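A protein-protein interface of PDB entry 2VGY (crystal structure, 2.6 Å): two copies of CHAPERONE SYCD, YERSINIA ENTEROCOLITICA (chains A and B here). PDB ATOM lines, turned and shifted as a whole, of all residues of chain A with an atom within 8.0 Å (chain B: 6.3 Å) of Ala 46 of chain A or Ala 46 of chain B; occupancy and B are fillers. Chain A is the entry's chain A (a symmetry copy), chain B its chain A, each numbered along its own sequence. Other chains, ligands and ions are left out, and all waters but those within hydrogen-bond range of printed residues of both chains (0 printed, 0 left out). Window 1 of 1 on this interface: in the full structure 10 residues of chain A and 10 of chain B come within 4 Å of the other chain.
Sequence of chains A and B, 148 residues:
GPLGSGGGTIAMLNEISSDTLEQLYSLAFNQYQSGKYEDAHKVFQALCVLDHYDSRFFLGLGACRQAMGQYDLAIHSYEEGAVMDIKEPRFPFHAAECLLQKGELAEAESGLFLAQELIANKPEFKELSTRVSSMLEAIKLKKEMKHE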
ATOM      1  N   LEU A  21       6.645 -15.286  -8.501  1.00  0.00           N
ATOM      2  CA  LEU A  21       6.801 -15.698  -9.885  1.00  0.00           C
ATOM      3  C   LEU A  21       7.194 -14.501 -10.737  1.00  0.00           C
ATOM      4  O   LEU A  21       7.964 -14.628 -11.688  1.00  0.00           O
ATOM      5  CB  LEU A  21       5.490 -16.287 -10.406  1.00  0.00           C
ATOM      6  CG  LEU A  21       4.831 -17.387  -9.569  1.00  0.00           C
ATOM      7  CD1 LEU A  21       3.441 -17.708 -10.098  1.00  0.00           C
ATOM      8  CD2 LEU A  21       5.695 -18.630  -9.556  1.00  0.00           C
ATOM      9  N   LEU A  24      10.886 -13.626  -9.932  1.00  0.00           N
ATOM     10  CA  LEU A  24      11.727 -14.600 -10.616  1.00  0.00           C
ATOM     11  C   LEU A  24      11.708 -14.361 -12.120  1.00  0.00           C
ATOM     12  O   LEU A  24      12.743 -14.426 -12.782  1.00  0.00           O
ATOM     13  CB  LEU A  24      11.247 -16.018 -10.310  1.00  0.00           C
ATOM     14  CG  LEU A  24      11.247 -16.415  -8.835  1.00  0.00           C
ATOM     15  CD1 LEU A  24      10.574 -17.767  -8.635  1.00  0.00           C
ATOM     16  CD2 LEU A  24      12.668 -16.433  -8.297  1.00  0.00           C
ATOM     17  N   LEU A  27      13.746 -11.470 -12.980  1.00  0.00           N
ATOM     18  CA  LEU A  27      15.151 -11.835 -12.865  1.00  0.00           C
ATOM     19  C   LEU A  27      15.621 -12.594 -14.097  1.00  0.00           C
ATOM     20  O   LEU A  27      16.644 -12.256 -14.694  1.00  0.00           O
ATOM     21  CB  LEU A  27      15.384 -12.689 -11.618  1.00  0.00           C
ATOM     22  CG  LEU A  27      16.759 -13.352 -11.557  1.00  0.00           C
ATOM     23  CD1 LEU A  27      17.859 -12.300 -11.539  1.00  0.00           C
ATOM     24  CD2 LEU A  27      16.862 -14.258 -10.346  1.00  0.00           C
ATOM     25  N   GLN A  31      18.400 -11.510 -16.933  1.00  0.00           N
ATOM     26  CA  GLN A  31      19.531 -12.379 -17.235  1.00  0.00           C
ATOM     27  C   GLN A  31      19.629 -12.654 -18.730  1.00  0.00           C
ATOM     28  O   GLN A  31      20.724 -12.678 -19.294  1.00  0.00           O
ATOM     29  CB  GLN A  31      19.419 -13.692 -16.463  1.00  0.00           C
ATOM     30  CG  GLN A  31      19.636 -13.549 -14.971  1.00  0.00           C
ATOM     31  CD  GLN A  31      19.263 -14.802 -14.212  1.00  0.00           C
ATOM     32  OE1 GLN A  31      18.350 -15.528 -14.603  1.00  0.00           O
ATOM     33  NE2 GLN A  31      19.965 -15.063 -13.118  1.00  0.00           N
ATOM     34  N   ASP A  39      21.788 -19.227 -17.052  1.00  0.00           N
ATOM     35  CA  ASP A  39      21.193 -18.900 -15.763  1.00  0.00           C
ATOM     36  C   ASP A  39      19.713 -18.588 -15.935  1.00  0.00           C
ATOM     37  O   ASP A  39      18.870 -19.097 -15.196  1.00  0.00           O
ATOM     38  CB  ASP A  39      21.907 -17.706 -15.126  1.00  0.00           C
ATOM     39  CG  ASP A  39      23.303 -18.047 -14.649  1.00  0.00           C
ATOM     40  OD1 ASP A  39      23.759 -19.183 -14.900  1.00  0.00           O
ATOM     41  OD2 ASP A  39      23.945 -17.178 -14.022  1.00  0.00           O
ATOM     42  N   ALA A  40      19.406 -17.744 -16.915  1.00  0.00           N
ATOM     43  CA  ALA A  40      18.023 -17.412 -17.234  1.00  0.00           C
ATOM     44  C   ALA A  40      17.242 -18.686 -17.525  1.00  0.00           C
ATOM     45  O   ALA A  40      16.090 -18.831 -17.123  1.00  0.00           O
ATOM     46  CB  ALA A  40      17.968 -16.464 -18.425  1.00  0.00           C
ATOM     47  N   HIS A  41      17.889 -19.612 -18.222  1.00  0.00           N
ATOM     48  CA  HIS A  41      17.287 -20.894 -18.555  1.00  0.00           C
ATOM     49  C   HIS A  41      16.892 -21.663 -17.299  1.00  0.00           C
ATOM     50  O   HIS A  41      15.806 -22.228 -17.226  1.00  0.00           O
ATOM     51  CB  HIS A  41      18.259 -21.721 -19.397  1.00  0.00           C
ATOM     52  CG  HIS A  41      17.743 -23.077 -19.763  1.00  0.00           C
ATOM     53  ND1 HIS A  41      17.781 -24.147 -18.894  1.00  0.00           N
ATOM     54  CD2 HIS A  41      17.188 -23.541 -20.907  1.00  0.00           C
ATOM     55  CE1 HIS A  41      17.267 -25.209 -19.486  1.00  0.00           C
ATOM     56  NE2 HIS A  41      16.898 -24.869 -20.707  1.00  0.00           N
ATOM     57  N   MLY A  42      17.781 -21.676 -16.310  1.00  0.00           N
ATOM     58  CA  MLY A  42      17.537 -22.393 -15.070  1.00  0.00           C
ATOM     59  CB  MLY A  42      18.769 -22.304 -14.173  1.00  0.00           C
ATOM     60  CG  MLY A  42      19.851 -23.269 -14.642  1.00  0.00           C
ATOM     61  CD  MLY A  42      21.227 -22.890 -14.105  1.00  0.00           C
ATOM     62  CE  MLY A  42      22.210 -24.026 -14.363  1.00  0.00           C
ATOM     63  NZ  MLY A  42      23.497 -23.579 -13.849  1.00  0.00           N
ATOM     64  CH1 MLY A  42      24.536 -24.554 -13.560  1.00  0.00           C
ATOM     65  CH2 MLY A  42      23.749 -22.164 -13.633  1.00  0.00           C
ATOM     66  C   MLY A  42      16.354 -21.816 -14.346  1.00  0.00           C
ATOM     67  O   MLY A  42      15.544 -22.582 -13.774  1.00  0.00           O
ATOM     68  N   VAL A  43      16.237 -20.491 -14.342  1.00  0.00           N
ATOM     69  CA  VAL A  43      15.148 -19.818 -13.640  1.00  0.00           C
ATOM     70  C   VAL A  43      13.817 -20.012 -14.360  1.00  0.00           C
ATOM     71  O   VAL A  43      12.805 -20.324 -13.732  1.00  0.00           O
ATOM     72  CB  VAL A  43      15.431 -18.311 -13.463  1.00  0.00           C
ATOM     73  CG1 VAL A  43      14.268 -17.628 -12.755  1.00  0.00           C
ATOM     74  CG2 VAL A  43      16.721 -18.102 -12.689  1.00  0.00           C
ATOM     75  N   PHE A  44      13.827 -19.831 -15.679  1.00  0.00           N
ATOM     76  CA  PHE A  44      12.626 -20.009 -16.491  1.00  0.00           C
ATOM     77  C   PHE A  44      12.082 -21.430 -16.384  1.00  0.00           C
ATOM     78  O   PHE A  44      10.872 -21.642 -16.296  1.00  0.00           O
ATOM     79  CB  PHE A  44      12.911 -19.677 -17.957  1.00  0.00           C
ATOM     80  CG  PHE A  44      12.772 -18.221 -18.287  1.00  0.00           C
ATOM     81  CD1 PHE A  44      11.587 -17.550 -18.031  1.00  0.00           C
ATOM     82  CD2 PHE A  44      13.817 -17.523 -18.869  1.00  0.00           C
ATOM     83  CE1 PHE A  44      11.454 -16.209 -18.335  1.00  0.00           C
ATOM     84  CE2 PHE A  44      13.689 -16.182 -19.177  1.00  0.00           C
ATOM     85  CZ  PHE A  44      12.506 -15.524 -18.910  1.00  0.00           C
ATOM     86  N   GLN A  45      12.992 -22.398 -16.392  1.00  0.00           N
ATOM     87  CA  GLN A  45      12.634 -23.805 -16.286  1.00  0.00           C
ATOM     88  C   GLN A  45      11.972 -24.077 -14.945  1.00  0.00           C
ATOM     89  O   GLN A  45      11.052 -24.888 -14.847  1.00  0.00           O
ATOM     90  CB  GLN A  45      13.880 -24.676 -16.440  1.00  0.00           C
ATOM     91  CG  GLN A  45      13.598 -26.105 -16.857  1.00  0.00           C
ATOM     92  CD  GLN A  45      14.850 -26.816 -17.337  1.00  0.00           C
ATOM     93  OE1 GLN A  45      15.967 -26.428 -16.992  1.00  0.00           O
ATOM     94  NE2 GLN A  45      14.672 -27.859 -18.137  1.00  0.00           N
ATOM     95  N   ALA A  46      12.446 -23.392 -13.911  1.00  0.00           N
ATOM     96  CA  ALA A  46      11.876 -23.537 -12.579  1.00  0.00           C
ATOM     97  C   ALA A  46      10.495 -22.895 -12.512  1.00  0.00           C
ATOM     98  O   ALA A  46       9.610 -23.379 -11.811  1.00  0.00           O
ATOM     99  CB  ALA A  46      12.797 -22.928 -11.540  1.00  0.00           C
ATOM    100  N   LEU A  47      10.321 -21.799 -13.243  1.00  0.00           N
ATOM    101  CA  LEU A  47       9.031 -21.126 -13.318  1.00  0.00           C
ATOM    102  C   LEU A  47       8.018 -22.012 -14.032  1.00  0.00           C
ATOM    103  O   LEU A  47       6.846 -22.053 -13.661  1.00  0.00           O
ATOM    104  CB  LEU A  47       9.163 -19.786 -14.045  1.00  0.00           C
ATOM    105  CG  LEU A  47       9.883 -18.670 -13.288  1.00  0.00           C
ATOM    106  CD1 LEU A  47      10.005 -17.422 -14.153  1.00  0.00           C
ATOM    107  CD2 LEU A  47       9.152 -18.356 -11.993  1.00  0.00           C
ATOM    108  N   CYS A  48       8.480 -22.724 -15.056  1.00  0.00           N
ATOM    109  CA  CYS A  48       7.622 -23.640 -15.800  1.00  0.00           C
ATOM    110  C   CYS A  48       7.073 -24.738 -14.893  1.00  0.00           C
ATOM    111  O   CYS A  48       6.107 -25.417 -15.237  1.00  0.00           O
ATOM    112  CB  CYS A  48       8.382 -24.259 -16.977  1.00  0.00           C
ATOM    113  SG  CYS A  48       8.697 -23.127 -18.351  1.00  0.00           S
ATOM    114  N   VAL A  49       7.699 -24.909 -13.734  1.00  0.00           N
ATOM    115  CA  VAL A  49       7.239 -25.886 -12.756  1.00  0.00           C
ATOM    116  C   VAL A  49       6.221 -25.257 -11.806  1.00  0.00           C
ATOM    117  O   VAL A  49       5.195 -25.859 -11.494  1.00  0.00           O
ATOM    118  CB  VAL A  49       8.412 -26.467 -11.945  1.00  0.00           C
ATOM    119  CG1 VAL A  49       7.894 -27.341 -10.814  1.00  0.00           C
ATOM    120  CG2 VAL A  49       9.343 -27.256 -12.853  1.00  0.00           C
ATOM    121  N   LEU A  50       6.515 -24.041 -11.360  1.00  0.00           N
ATOM    122  CA  LEU A  50       5.643 -23.332 -10.430  1.00  0.00           C
ATOM    123  C   LEU A  50       4.282 -23.039 -11.050  1.00  0.00           C
ATOM    124  O   LEU A  50       3.264 -23.026 -10.361  1.00  0.00           O
ATOM    125  CB  LEU A  50       6.302 -22.030  -9.977  1.00  0.00           C
ATOM    126  CG  LEU A  50       7.735 -22.183  -9.465  1.00  0.00           C
ATOM    127  CD1 LEU A  50       8.315 -20.841  -9.055  1.00  0.00           C
ATOM    128  CD2 LEU A  50       7.777 -23.160  -8.308  1.00  0.00           C
ATOM    129  N   ASP A  51       4.276 -22.805 -12.359  1.00  0.00           N
ATOM    130  CA  ASP A  51       3.050 -22.510 -13.085  1.00  0.00           C
ATOM    131  C   ASP A  51       3.200 -22.947 -14.535  1.00  0.00           C
ATOM    132  O   ASP A  51       3.556 -22.145 -15.398  1.00  0.00           O
ATOM    133  CB  ASP A  51       2.742 -21.013 -13.015  1.00  0.00           C
ATOM    134  CG  ASP A  51       1.366 -20.676 -13.554  1.00  0.00           C
ATOM    135  OD1 ASP A  51       0.525 -21.594 -13.661  1.00  0.00           O
ATOM    136  OD2 ASP A  51       1.124 -19.490 -13.863  1.00  0.00           O
ATOM    137  N   HIS A  52       2.930 -24.222 -14.801  1.00  0.00           N
ATOM    138  CA  HIS A  52       3.134 -24.781 -16.136  1.00  0.00           C
ATOM    139  C   HIS A  52       2.008 -24.438 -17.107  1.00  0.00           C
ATOM    140  O   HIS A  52       1.925 -25.007 -18.197  1.00  0.00           O
ATOM    141  CB  HIS A  52       3.341 -26.296 -16.069  1.00  0.00           C
ATOM    142  CG  HIS A  52       2.297 -27.014 -15.275  1.00  0.00           C
ATOM    143  ND1 HIS A  52       1.225 -27.652 -15.859  1.00  0.00           N
ATOM    144  CD2 HIS A  52       2.164 -27.201 -13.938  1.00  0.00           C
ATOM    145  CE1 HIS A  52       0.473 -28.198 -14.919  1.00  0.00           C
ATOM    146  NE2 HIS A  52       1.023 -27.939 -13.745  1.00  0.00           N
ATOM    147  N   PHE A  57       6.623 -18.222 -19.422  1.00  0.00           N
ATOM    148  CA  PHE A  57       7.789 -18.983 -18.993  1.00  0.00           C
ATOM    149  C   PHE A  57       8.306 -19.880 -20.107  1.00  0.00           C
ATOM    150  O   PHE A  57       9.510 -20.090 -20.237  1.00  0.00           O
ATOM    151  CB  PHE A  57       7.469 -19.825 -17.754  1.00  0.00           C
ATOM    152  CG  PHE A  57       6.805 -19.057 -16.644  1.00  0.00           C
ATOM    153  CD1 PHE A  57       7.037 -17.702 -16.481  1.00  0.00           C
ATOM    154  CD2 PHE A  57       5.965 -19.698 -15.749  1.00  0.00           C
ATOM    155  CE1 PHE A  57       6.426 -16.996 -15.459  1.00  0.00           C
ATOM    156  CE2 PHE A  57       5.357 -18.999 -14.723  1.00  0.00           C
ATOM    157  CZ  PHE A  57       5.588 -17.646 -14.578  1.00  0.00           C
ATOM    158  N   LEU A  61      11.906 -19.580 -21.715  1.00  0.00           N
ATOM    159  CA  LEU A  61      12.747 -20.768 -21.750  1.00  0.00           C
ATOM    160  C   LEU A  61      13.158 -21.102 -23.180  1.00  0.00           C
ATOM    161  O   LEU A  61      14.324 -21.379 -23.450  1.00  0.00           O
ATOM    162  CB  LEU A  61      12.007 -21.953 -21.132  1.00  0.00           C
ATOM    163  CG  LEU A  61      12.748 -23.288 -21.114  1.00  0.00           C
ATOM    164  CD1 LEU A  61      14.044 -23.178 -20.328  1.00  0.00           C
ATOM    165  CD2 LEU A  61      11.861 -24.356 -20.525  1.00  0.00           C
ATOM    166  N   HIS B  41      14.753 -31.107  -9.380  1.00  0.00           N
ATOM    167  CA  HIS B  41      16.011 -30.753 -10.022  1.00  0.00           C
ATOM    168  C   HIS B  41      15.955 -29.347 -10.610  1.00  0.00           C
ATOM    169  O   HIS B  41      16.891 -28.568 -10.457  1.00  0.00           O
ATOM    170  CB  HIS B  41      16.339 -31.769 -11.115  1.00  0.00           C
ATOM    171  CG  HIS B  41      17.602 -31.472 -11.860  1.00  0.00           C
ATOM    172  ND1 HIS B  41      17.664 -30.544 -12.879  1.00  0.00           N
ATOM    173  CD2 HIS B  41      18.848 -31.987 -11.744  1.00  0.00           C
ATOM    174  CE1 HIS B  41      18.895 -30.498 -13.353  1.00  0.00           C
ATOM    175  NE2 HIS B  41      19.634 -31.362 -12.682  1.00  0.00           N
ATOM    176  N   MLY B  42      14.851 -29.027 -11.276  1.00  0.00           N
ATOM    177  CA  MLY B  42      14.684 -27.728 -11.905  1.00  0.00           C
ATOM    178  CB  MLY B  42      13.365 -27.693 -12.672  1.00  0.00           C
ATOM    179  CG  MLY B  42      13.487 -28.437 -13.996  1.00  0.00           C
ATOM    180  CD  MLY B  42      12.127 -28.837 -14.556  1.00  0.00           C
ATOM    181  CE  MLY B  42      12.284 -29.317 -15.994  1.00  0.00           C
ATOM    182  NZ  MLY B  42      10.955 -29.704 -16.446  1.00  0.00           N
ATOM    183  CH1 MLY B  42      10.678 -29.809 -17.868  1.00  0.00           C
ATOM    184  CH2 MLY B  42       9.908 -29.993 -15.479  1.00  0.00           C
ATOM    185  C   MLY B  42      14.688 -26.635 -10.875  1.00  0.00           C
ATOM    186  O   MLY B  42      15.278 -25.557 -11.119  1.00  0.00           O
ATOM    187  N   VAL B  43      14.038 -26.873  -9.739  1.00  0.00           N
ATOM    188  CA  VAL B  43      13.945 -25.871  -8.683  1.00  0.00           C
ATOM    189  C   VAL B  43      15.283 -25.686  -7.972  1.00  0.00           C
ATOM    190  O   VAL B  43      15.718 -24.557  -7.742  1.00  0.00           O
ATOM    191  CB  VAL B  43      12.852 -26.230  -7.653  1.00  0.00           C
ATOM    192  CG1 VAL B  43      12.795 -25.184  -6.548  1.00  0.00           C
ATOM    193  CG2 VAL B  43      11.502 -26.353  -8.339  1.00  0.00           C
ATOM    194  N   PHE B  44      15.929 -26.798  -7.630  1.00  0.00           N
ATOM    195  CA  PHE B  44      17.230 -26.760  -6.965  1.00  0.00           C
ATOM    196  C   PHE B  44      18.276 -26.050  -7.820  1.00  0.00           C
ATOM    197  O   PHE B  44      19.087 -25.274  -7.314  1.00  0.00           O
ATOM    198  CB  PHE B  44      17.709 -28.176  -6.636  1.00  0.00           C
ATOM    199  CG  PHE B  44      17.192 -28.703  -5.331  1.00  0.00           C
ATOM    200  CD1 PHE B  44      17.413 -28.007  -4.153  1.00  0.00           C
ATOM    201  CD2 PHE B  44      16.500 -29.901  -5.275  1.00  0.00           C
ATOM    202  CE1 PHE B  44      16.942 -28.490  -2.949  1.00  0.00           C
ATOM    203  CE2 PHE B  44      16.027 -30.389  -4.071  1.00  0.00           C
ATOM    204  CZ  PHE B  44      16.248 -29.683  -2.907  1.00  0.00           C
ATOM    205  N   GLN B  45      18.244 -26.327  -9.118  1.00  0.00           N
ATOM    206  CA  GLN B  45      19.168 -25.723 -10.067  1.00  0.00           C
ATOM    207  C   GLN B  45      18.961 -24.218 -10.113  1.00  0.00           C
ATOM    208  O   GLN B  45      19.913 -23.453 -10.259  1.00  0.00           O
ATOM    209  CB  GLN B  45      18.960 -26.324 -11.456  1.00  0.00           C
ATOM    210  CG  GLN B  45      20.148 -26.177 -12.386  1.00  0.00           C
ATOM    211  CD  GLN B  45      20.034 -27.080 -13.601  1.00  0.00           C
ATOM    212  OE1 GLN B  45      18.937 -27.497 -13.976  1.00  0.00           O
ATOM    213  NE2 GLN B  45      21.166 -27.389 -14.220  1.00  0.00           N
ATOM    214  N   ALA B  46      17.707 -23.799  -9.988  1.00  0.00           N
ATOM    215  CA  ALA B  46      17.378 -22.380  -9.982  1.00  0.00           C
ATOM    216  C   ALA B  46      17.844 -21.725  -8.687  1.00  0.00           C
ATOM    217  O   ALA B  46      18.253 -20.566  -8.681  1.00  0.00           O
ATOM    218  CB  ALA B  46      15.887 -22.181 -10.173  1.00  0.00           C
ATOM    219  N   LEU B  47      17.773 -22.473  -7.592  1.00  0.00           N
ATOM    220  CA  LEU B  47      18.246 -21.989  -6.302  1.00  0.00           C
ATOM    221  C   LEU B  47      19.758 -21.811  -6.331  1.00  0.00           C
ATOM    222  O   LEU B  47      20.293 -20.865  -5.753  1.00  0.00           O
ATOM    223  CB  LEU B  47      17.851 -22.956  -5.185  1.00  0.00           C
ATOM    224  CG  LEU B  47      16.371 -22.994  -4.809  1.00  0.00           C
ATOM    225  CD1 LEU B  47      16.110 -24.047  -3.738  1.00  0.00           C
ATOM    226  CD2 LEU B  47      15.913 -21.625  -4.336  1.00  0.00           C
ATOM    227  N   CYS B  48      20.444 -22.725  -7.013  1.00  0.00           N
ATOM    228  CA  CYS B  48      21.894 -22.648  -7.152  1.00  0.00           C
ATOM    229  C   CYS B  48      22.312 -21.365  -7.864  1.00  0.00           C
ATOM    230  O   CYS B  48      23.473 -20.962  -7.809  1.00  0.00           O
ATOM    231  CB  CYS B  48      22.432 -23.868  -7.905  1.00  0.00           C
ATOM    232  SG  CYS B  48      22.407 -25.410  -6.962  1.00  0.00           S
ATOM    233  N   VAL B  49      21.358 -20.729  -8.534  1.00  0.00           N
ATOM    234  CA  VAL B  49      21.615 -19.464  -9.210  1.00  0.00           C
ATOM    235  C   VAL B  49      21.361 -18.290  -8.268  1.00  0.00           C
ATOM    236  O   VAL B  49      22.143 -17.342  -8.216  1.00  0.00           O
ATOM    237  CB  VAL B  49      20.745 -19.311 -10.471  1.00  0.00           C
ATOM    238  CG1 VAL B  49      20.894 -17.916 -11.054  1.00  0.00           C
ATOM    239  CG2 VAL B  49      21.116 -20.369 -11.501  1.00  0.00           C
ATOM    240  N   LEU B  50      20.265 -18.369  -7.521  1.00  0.00           N
ATOM    241  CA  LEU B  50      19.888 -17.308  -6.592  1.00  0.00           C
ATOM    242  C   LEU B  50      20.922 -17.139  -5.486  1.00  0.00           C
ATOM    243  O   LEU B  50      21.151 -16.032  -5.000  1.00  0.00           O
ATOM    244  CB  LEU B  50      18.517 -17.601  -5.986  1.00  0.00           C
ATOM    245  CG  LEU B  50      17.424 -17.930  -7.004  1.00  0.00           C
ATOM    246  CD1 LEU B  50      16.104 -18.224  -6.314  1.00  0.00           C
ATOM    247  CD2 LEU B  50      17.269 -16.793  -7.993  1.00  0.00           C
ATOM    248  N   ASP B  51      21.544 -18.246  -5.095  1.00  0.00           N
ATOM    249  CA  ASP B  51      22.555 -18.234  -4.047  1.00  0.00           C
ATOM    250  C   ASP B  51      23.526 -19.387  -4.265  1.00  0.00           C
ATOM    251  O   ASP B  51      23.362 -20.461  -3.689  1.00  0.00           O
ATOM    252  CB  ASP B  51      21.893 -18.357  -2.673  1.00  0.00           C
ATOM    253  CG  ASP B  51      22.865 -18.123  -1.535  1.00  0.00           C
ATOM    254  OD1 ASP B  51      23.944 -17.542  -1.780  1.00  0.00           O
ATOM    255  OD2 ASP B  51      22.547 -18.515  -0.392  1.00  0.00           O
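Leu 27 of chain A touches Leu 50 of chain B.
Val 49 of chain B touches Gln 31 of chain A.
MLY 42 of chain B touches MLY 42 of chain A.
MLY 42 of chain A touches Gln 45 of chain B (CE to NE2, 3.5 Å).
MLY 42 of chain A touches Ala 46 of chain B (O to CB, 3.6 Å).
CD of MLY 42 of chain A touches CG2 of Val 49 of chain B, at 3.6 Å.
MLY 42 of chain B touches Gln 45 of chain A.
Ala 46 of chain A touches MLY 42 of chain B.
Ala 46 of chain B touches Ala 46 of chain A (CB to CB, 3.5 Å).
Val 49 of chain A touches MLY 42 of chain B.
OE1 of Gln 31 of chain A sits close to N of Ala 40 of chain A (3.4 Å).
ND1 of His 41 of chain B sits close to OE1 of Gln 45 of chain B (3.5 Å).
The side-chain amide oxygen (OE1) of Gln 45 of chain A lies close to a ring nitrogen (ND1) of His 41 of chain A (3.5 Å).
MLY 42 of chain A touches its own counterpart, MLY 42 of chain B.
MLY 42 of chain A touches Gln 45 of chain B, and with the chains exchanged Gln 45 of chain A touches MLY 42 of chain B.
MLY 42 of chain A touches Ala 46 of chain B, and with the chains exchanged Ala 46 of chain A touches MLY 42 of chain B.
MLY 42 of chain A touches Val 49 of chain B, and with the chains exchanged Val 49 of chain A touches MLY 42 of chain B.
Ala 46 of chain A touches just these residues of chain B: MLY 42 and Ala 46.
Ala 46 of chain B touches just these residues of chain A: MLY 42 and Ala 46.
Printed residues of chain B within 4 Å of MLY 42 of chain A: MLY 42, Gln 45, Ala 46 and Val 49.
Of the printed residues of chain B, Val 49 of chain A touches MLY 42.
Leu 50 of chain A touches none of the printed residues of chain B.
Leu 24 of chain A touches none of the printed residues of chain B.
The nearest residue of chain B that does not touch Ala 46 of chain A is Val 43 of chain B (4.3 Å).
The nearest printed residue of chain B that does not touch Gln 31 of chain A is Leu 50 of chain B (6.0 Å).
Hydrophobic or aromatic side chains of chain A within 4 Å of the printed part of chain B: Leu 27, Ala 46 and Val 49.
Of the 11 printed residues of chain B, 5 touch a printed residue of chain A.
Printed residues of chain B that touch a printed residue of chain A: MLY 42, Gln 45, Ala 46, Val 49 and Leu 50.
Along chain B the printed residues that touch a printed residue of chain A span positions 42 to 50.
Among the printed residues, 10 pairs touch across the chains.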
